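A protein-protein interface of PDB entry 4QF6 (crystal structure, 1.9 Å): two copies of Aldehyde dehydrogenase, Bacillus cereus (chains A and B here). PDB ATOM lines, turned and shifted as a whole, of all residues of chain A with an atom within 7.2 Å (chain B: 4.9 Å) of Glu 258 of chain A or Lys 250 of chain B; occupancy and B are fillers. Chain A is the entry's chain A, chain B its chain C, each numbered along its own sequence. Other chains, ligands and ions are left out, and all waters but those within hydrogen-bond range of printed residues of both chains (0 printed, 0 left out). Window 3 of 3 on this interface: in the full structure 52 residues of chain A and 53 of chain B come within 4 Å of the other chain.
The side-chain amino group (NZ) of Lys 250 of chain B sits close to the backbone carbonyl oxygen (O) of Glu 258 of chain A (3.4 Å).
SD of Met 259 of chain A sits close to NZ of Lys 261 of chain A (3.5 Å).
Among the printed residues, merely in contact across the chains: Arg 254 of chain A with Arg 254 of chain B (3.8 Å), Ala 257 of chain A with Lys 250 of chain B (3.4 Å), Ala 257 of chain A with Met 253 of chain B (3.6 Å), Met 259 of chain A with Gln 468 of chain B (3.7 Å), Ile 260 of chain A with Lys 250 of chain B (3.7 Å), Ile 260 of chain A with Met 253 of chain B (3.7 Å) and Ile 260 of chain A with Gln 468 of chain B (3.8 Å).
Of chain B, only Lys 250 (3.2 Å) comes within 4 Å of Glu 258 of chain A. Lys 250 of chain B touches three residues of chain A. No residue of chain A comes within 4 Å of Gly 249 of chain B. Of the printed residues of chain A, Met 253 of chain B touches Ala 257 (3.6 Å) and Ile 260 (3.7 Å). Of the printed residues of chain B, Ala 257 of chain A touches Lys 250 and Met 253. Ile 252 of chain B touches none of the printed residues of chain A. The nearest residue of chain A that does not touch Lys 250 of chain B is Met 259 of chain A (4.9 Å).
Hydrophobic or aromatic side chains of chain A within 4 Å of the printed part of chain B: Ala 257 and Ile 260. Printed residues of chain B that touch a printed residue of chain A: Lys 250, Met 253, Arg 254 and Gln 468.
Arg 254 of chain B touches its own counterpart, Arg 254 of chain A. Of the 8 pairs that touch across the chains among the printed residues, 1 has its exchanged pair printed and touching as well.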
ATOM      1  N   VAL A 232       2.613   9.068 -25.420  1.00  0.00           N
ATOM      2  CA  VAL A 232       3.372  10.226 -24.791  1.00  0.00           C
ATOM      3  C   VAL A 232       2.544  10.842 -23.654  1.00  0.00           C
ATOM      4  O   VAL A 232       3.066  11.198 -22.595  1.00  0.00           O
ATOM      5  CB  VAL A 232       3.714  11.253 -25.851  1.00  0.00           C
ATOM      6  CG1 VAL A 232       4.259  12.533 -25.254  1.00  0.00           C
ATOM      7  CG2 VAL A 232       4.688  10.701 -26.867  1.00  0.00           C
ATOM      8  N   ASN A 233       1.237  10.926 -23.879  1.00  0.00           N
ATOM      9  CA  ASN A 233       0.299  11.559 -22.928  1.00  0.00           C
ATOM     10  C   ASN A 233      -0.378  10.660 -21.909  1.00  0.00           C
ATOM     11  O   ASN A 233      -1.141  11.175 -21.093  1.00  0.00           O
ATOM     12  CB  ASN A 233      -0.708  12.401 -23.697  1.00  0.00           C
ATOM     13  CG  ASN A 233      -0.036  13.502 -24.464  1.00  0.00           C
ATOM     14  OD1 ASN A 233       0.717  14.259 -23.885  1.00  0.00           O
ATOM     15  ND2 ASN A 233      -0.297  13.618 -25.744  1.00  0.00           N
ATOM     16  N   MET A 253       9.544  15.661 -24.368  1.00  0.00           N
ATOM     17  CA  MET A 253      10.059  16.253 -23.144  1.00  0.00           C
ATOM     18  C   MET A 253       9.137  17.277 -22.560  1.00  0.00           C
ATOM     19  O   MET A 253       8.974  17.343 -21.344  1.00  0.00           O
ATOM     20  CB  MET A 253      11.445  16.859 -23.335  1.00  0.00           C
ATOM     21  CG  MET A 253      12.399  16.551 -22.128  1.00  0.00           C
ATOM     22  SD  MET A 253      14.079  17.240 -22.256  1.00  0.00           S
ATOM     23  CE  MET A 253      14.146  16.865 -24.022  1.00  0.00           C
ATOM     24  N   ARG A 254       8.518  18.096 -23.418  1.00  0.00           N
ATOM     25  CA  ARG A 254       7.601  19.119 -22.959  1.00  0.00           C
ATOM     26  C   ARG A 254       6.384  18.419 -22.294  1.00  0.00           C
ATOM     27  O   ARG A 254       5.982  18.760 -21.170  1.00  0.00           O
ATOM     28  CB  ARG A 254       7.300  20.021 -24.209  1.00  0.00           C
ATOM     29  CG  ARG A 254       6.539  21.312 -24.100  1.00  0.00           C
ATOM     30  CD  ARG A 254       6.061  21.817 -25.479  1.00  0.00           C
ATOM     31  NE  ARG A 254       7.203  21.939 -26.374  1.00  0.00           N
ATOM     32  CZ  ARG A 254       7.345  21.419 -27.620  1.00  0.00           C
ATOM     33  NH1 ARG A 254       6.363  20.841 -28.319  1.00  0.00           N
ATOM     34  NH2 ARG A 254       8.477  21.597 -28.212  1.00  0.00           N
ATOM     35  N   GLN A 255       5.815  17.410 -22.963  1.00  0.00           N
ATOM     36  CA  GLN A 255       4.647  16.712 -22.449  1.00  0.00           C
ATOM     37  C   GLN A 255       4.925  15.901 -21.178  1.00  0.00           C
ATOM     38  O   GLN A 255       4.031  15.699 -20.328  1.00  0.00           O
ATOM     39  CB  GLN A 255       4.092  15.741 -23.487  1.00  0.00           C
ATOM     40  CG  GLN A 255       3.520  16.365 -24.760  1.00  0.00           C
ATOM     41  CD  GLN A 255       2.520  17.454 -24.454  1.00  0.00           C
ATOM     42  OE1 GLN A 255       2.879  18.605 -24.386  1.00  0.00           O
ATOM     43  NE2 GLN A 255       1.280  17.087 -24.227  1.00  0.00           N
ATOM     44  N   SER A 256       6.137  15.378 -21.080  1.00  0.00           N
ATOM     45  CA  SER A 256       6.534  14.620 -19.925  1.00  0.00           C
ATOM     46  C   SER A 256       6.681  15.461 -18.654  1.00  0.00           C
ATOM     47  O   SER A 256       6.615  14.935 -17.585  1.00  0.00           O
ATOM     48  CB  SER A 256       7.851  13.904 -20.207  1.00  0.00           C
ATOM     49  OG  SER A 256       7.649  12.956 -21.240  1.00  0.00           O
ATOM     50  N   ALA A 257       6.914  16.747 -18.782  1.00  0.00           N
ATOM     51  CA  ALA A 257       6.897  17.649 -17.617  1.00  0.00           C
ATOM     52  C   ALA A 257       5.665  17.459 -16.754  1.00  0.00           C
ATOM     53  O   ALA A 257       5.763  17.462 -15.515  1.00  0.00           O
ATOM     54  CB  ALA A 257       6.919  19.115 -18.065  1.00  0.00           C
ATOM     55  N   GLU A 258       4.487  17.363 -17.386  1.00  0.00           N
ATOM     56  CA  GLU A 258       3.231  17.372 -16.604  1.00  0.00           C
ATOM     57  C   GLU A 258       3.199  16.278 -15.593  1.00  0.00           C
ATOM     58  O   GLU A 258       2.542  16.418 -14.590  1.00  0.00           O
ATOM     59  CB  GLU A 258       1.960  17.284 -17.463  1.00  0.00           C
ATOM     60  CG  GLU A 258       1.864  18.366 -18.505  1.00  0.00           C
ATOM     61  CD  GLU A 258       0.761  18.086 -19.539  1.00  0.00           C
ATOM     62  OE1 GLU A 258       0.467  18.978 -20.347  1.00  0.00           O
ATOM     63  OE2 GLU A 258       0.167  16.982 -19.544  1.00  0.00           O
ATOM     64  N   MET A 259       3.888  15.163 -15.873  1.00  0.00           N
ATOM     65  CA  MET A 259       3.879  14.051 -14.952  1.00  0.00           C
ATOM     66  C   MET A 259       5.260  13.800 -14.306  1.00  0.00           C
ATOM     67  O   MET A 259       5.425  12.801 -13.641  1.00  0.00           O
ATOM     68  CB  MET A 259       3.364  12.766 -15.646  1.00  0.00           C
ATOM     69  CG  MET A 259       2.033  12.857 -16.335  1.00  0.00           C
ATOM     70  SD  MET A 259       1.881  11.585 -17.625  1.00  0.00           S
ATOM     71  CE  MET A 259       2.404  12.379 -19.170  1.00  0.00           C
ATOM     72  N   ILE A 260       6.217  14.708 -14.445  1.00  0.00           N
ATOM     73  CA  ILE A 260       7.589  14.508 -13.848  1.00  0.00           C
ATOM     74  C   ILE A 260       8.163  13.119 -14.237  1.00  0.00           C
ATOM     75  O   ILE A 260       8.835  12.361 -13.409  1.00  0.00           O
ATOM     76  CB  ILE A 260       7.626  14.699 -12.326  1.00  0.00           C
ATOM     77  CG1 ILE A 260       6.824  15.947 -11.900  1.00  0.00           C
ATOM     78  CG2 ILE A 260       9.067  14.942 -11.836  1.00  0.00           C
ATOM     79  CD1 ILE A 260       7.382  17.230 -12.505  1.00  0.00           C
ATOM     80  N   LYS A 261       7.972  12.843 -15.531  1.00  0.00           N
ATOM     81  CA  LYS A 261       8.301  11.554 -16.141  1.00  0.00           C
ATOM     82  C   LYS A 261       9.678  11.515 -16.754  1.00  0.00           C
ATOM     83  O   LYS A 261      10.071  12.413 -17.528  1.00  0.00           O
ATOM     84  CB  LYS A 261       7.225  11.224 -17.149  1.00  0.00           C
ATOM     85  CG  LYS A 261       7.299   9.817 -17.648  1.00  0.00           C
ATOM     86  CD  LYS A 261       6.210   9.425 -18.652  1.00  0.00           C
ATOM     87  CE  LYS A 261       4.854  10.024 -18.393  1.00  0.00           C
ATOM     88  NZ  LYS A 261       3.873   9.195 -19.154  1.00  0.00           N
ATOM     89  N   THR B 246       6.884  22.085  -7.357  1.00  0.00           N
ATOM     90  CA  THR B 246       6.506  21.312  -8.522  1.00  0.00           C
ATOM     91  C   THR B 246       6.230  22.177  -9.683  1.00  0.00           C
ATOM     92  O   THR B 246       6.658  21.875 -10.750  1.00  0.00           O
ATOM     93  CB  THR B 246       5.308  20.393  -8.215  1.00  0.00           C
ATOM     94  OG1 THR B 246       5.601  19.692  -7.017  1.00  0.00           O
ATOM     95  CG2 THR B 246       5.112  19.344  -9.310  1.00  0.00           C
ATOM     96  N   VAL B 247       5.561  23.291  -9.475  1.00  0.00           N
ATOM     97  CA  VAL B 247       5.118  24.123 -10.591  1.00  0.00           C
ATOM     98  C   VAL B 247       6.343  24.667 -11.352  1.00  0.00           C
ATOM     99  O   VAL B 247       6.401  24.631 -12.582  1.00  0.00           O
ATOM    100  CB  VAL B 247       4.139  25.274 -10.115  1.00  0.00           C
ATOM    101  CG1 VAL B 247       3.116  25.596 -11.188  1.00  0.00           C
ATOM    102  CG2 VAL B 247       3.448  24.896  -8.816  1.00  0.00           C
ATOM    103  N   THR B 248       7.375  25.065 -10.594  1.00  0.00           N
ATOM    104  CA  THR B 248       8.630  25.446 -11.161  1.00  0.00           C
ATOM    105  C   THR B 248       9.287  24.169 -11.770  1.00  0.00           C
ATOM    106  O   THR B 248       9.923  24.313 -12.783  1.00  0.00           O
ATOM    107  CB  THR B 248       9.574  26.141 -10.122  1.00  0.00           C
ATOM    108  OG1 THR B 248       8.978  27.387  -9.655  1.00  0.00           O
ATOM    109  CG2 THR B 248      10.895  26.528 -10.756  1.00  0.00           C
ATOM    110  N   GLY B 249       9.255  23.008 -11.076  1.00  0.00           N
ATOM    111  CA  GLY B 249       9.910  21.824 -11.616  1.00  0.00           C
ATOM    112  C   GLY B 249       9.371  21.492 -13.024  1.00  0.00           C
ATOM    113  O   GLY B 249      10.133  21.253 -13.990  1.00  0.00           O
ATOM    114  N   LYS B 250       8.041  21.470 -13.111  1.00  0.00           N
ATOM    115  CA  LYS B 250       7.371  21.403 -14.413  1.00  0.00           C
ATOM    116  C   LYS B 250       7.833  22.446 -15.422  1.00  0.00           C
ATOM    117  O   LYS B 250       8.107  22.085 -16.623  1.00  0.00           O
ATOM    118  CB  LYS B 250       5.835  21.423 -14.223  1.00  0.00           C
ATOM    119  CG  LYS B 250       5.357  20.144 -13.547  1.00  0.00           C
ATOM    120  CD  LYS B 250       3.857  20.086 -13.438  1.00  0.00           C
ATOM    121  CE  LYS B 250       3.455  18.840 -12.685  1.00  0.00           C
ATOM    122  NZ  LYS B 250       2.024  18.983 -12.482  1.00  0.00           N
ATOM    123  N   TYR B 251       7.905  23.726 -14.998  1.00  0.00           N
ATOM    124  CA  TYR B 251       8.385  24.818 -15.885  1.00  0.00           C
ATOM    125  C   TYR B 251       9.773  24.461 -16.353  1.00  0.00           C
ATOM    126  O   TYR B 251      10.048  24.541 -17.526  1.00  0.00           O
ATOM    127  CB  TYR B 251       8.366  26.243 -15.217  1.00  0.00           C
ATOM    128  CG  TYR B 251       9.069  27.370 -15.969  1.00  0.00           C
ATOM    129  CD1 TYR B 251      10.371  27.816 -15.622  1.00  0.00           C
ATOM    130  CD2 TYR B 251       8.422  28.037 -16.959  1.00  0.00           C
ATOM    131  CE1 TYR B 251      10.970  28.881 -16.317  1.00  0.00           C
ATOM    132  CE2 TYR B 251       8.991  29.116 -17.635  1.00  0.00           C
ATOM    133  CZ  TYR B 251      10.270  29.509 -17.337  1.00  0.00           C
ATOM    134  OH  TYR B 251      10.829  30.496 -18.107  1.00  0.00           O
ATOM    135  N   ILE B 252      10.620  23.993 -15.428  1.00  0.00           N
ATOM    136  CA  ILE B 252      11.968  23.707 -15.782  1.00  0.00           C
ATOM    137  C   ILE B 252      12.105  22.617 -16.811  1.00  0.00           C
ATOM    138  O   ILE B 252      12.867  22.760 -17.758  1.00  0.00           O
ATOM    139  CB  ILE B 252      12.788  23.433 -14.539  1.00  0.00           C
ATOM    140  CG1 ILE B 252      12.940  24.789 -13.821  1.00  0.00           C
ATOM    141  CG2 ILE B 252      14.133  22.882 -14.949  1.00  0.00           C
ATOM    142  CD1 ILE B 252      13.494  24.640 -12.402  1.00  0.00           C
ATOM    143  N   MET B 253      11.317  21.574 -16.648  1.00  0.00           N
ATOM    144  CA  MET B 253      11.358  20.496 -17.565  1.00  0.00           C
ATOM    145  C   MET B 253      10.844  20.929 -18.914  1.00  0.00           C
ATOM    146  O   MET B 253      11.429  20.574 -19.967  1.00  0.00           O
ATOM    147  CB  MET B 253      10.612  19.261 -17.065  1.00  0.00           C
ATOM    148  CG  MET B 253      11.466  17.964 -17.164  1.00  0.00           C
ATOM    149  SD  MET B 253      10.591  16.378 -16.932  1.00  0.00           S
ATOM    150  CE  MET B 253       9.760  17.064 -15.520  1.00  0.00           C
ATOM    151  N   ARG B 254       9.829  21.779 -18.905  1.00  0.00           N
ATOM    152  CA  ARG B 254       9.278  22.275 -20.153  1.00  0.00           C
ATOM    153  C   ARG B 254      10.272  23.090 -20.932  1.00  0.00           C
ATOM    154  O   ARG B 254      10.518  22.810 -22.101  1.00  0.00           O
ATOM    155  CB  ARG B 254       8.004  23.086 -19.832  1.00  0.00           C
ATOM    156  CG  ARG B 254       6.927  23.136 -20.841  1.00  0.00           C
ATOM    157  CD  ARG B 254       5.841  24.136 -20.398  1.00  0.00           C
ATOM    158  NE  ARG B 254       5.287  23.785 -19.108  1.00  0.00           N
ATOM    159  CZ  ARG B 254       5.194  24.542 -18.002  1.00  0.00           C
ATOM    160  NH1 ARG B 254       5.509  25.838 -17.933  1.00  0.00           N
ATOM    161  NH2 ARG B 254       4.723  23.957 -16.917  1.00  0.00           N
ATOM    162  N   GLN B 468       5.865  12.025  -8.952  1.00  0.00           N
ATOM    163  CA  GLN B 468       6.040  13.419  -9.112  1.00  0.00           C
ATOM    164  C   GLN B 468       6.868  14.020  -8.019  1.00  0.00           C
ATOM    165  O   GLN B 468       6.906  15.234  -7.897  1.00  0.00           O
ATOM    166  CB  GLN B 468       4.679  14.102  -9.294  1.00  0.00           C
ATOM    167  CG  GLN B 468       3.843  13.447 -10.337  1.00  0.00           C
ATOM    168  CD  GLN B 468       2.676  14.327 -10.763  1.00  0.00           C
ATOM    169  OE1 GLN B 468       2.648  15.526 -10.500  1.00  0.00           O
ATOM    170  NE2 GLN B 468       1.753  13.741 -11.457  1.00  0.00           N
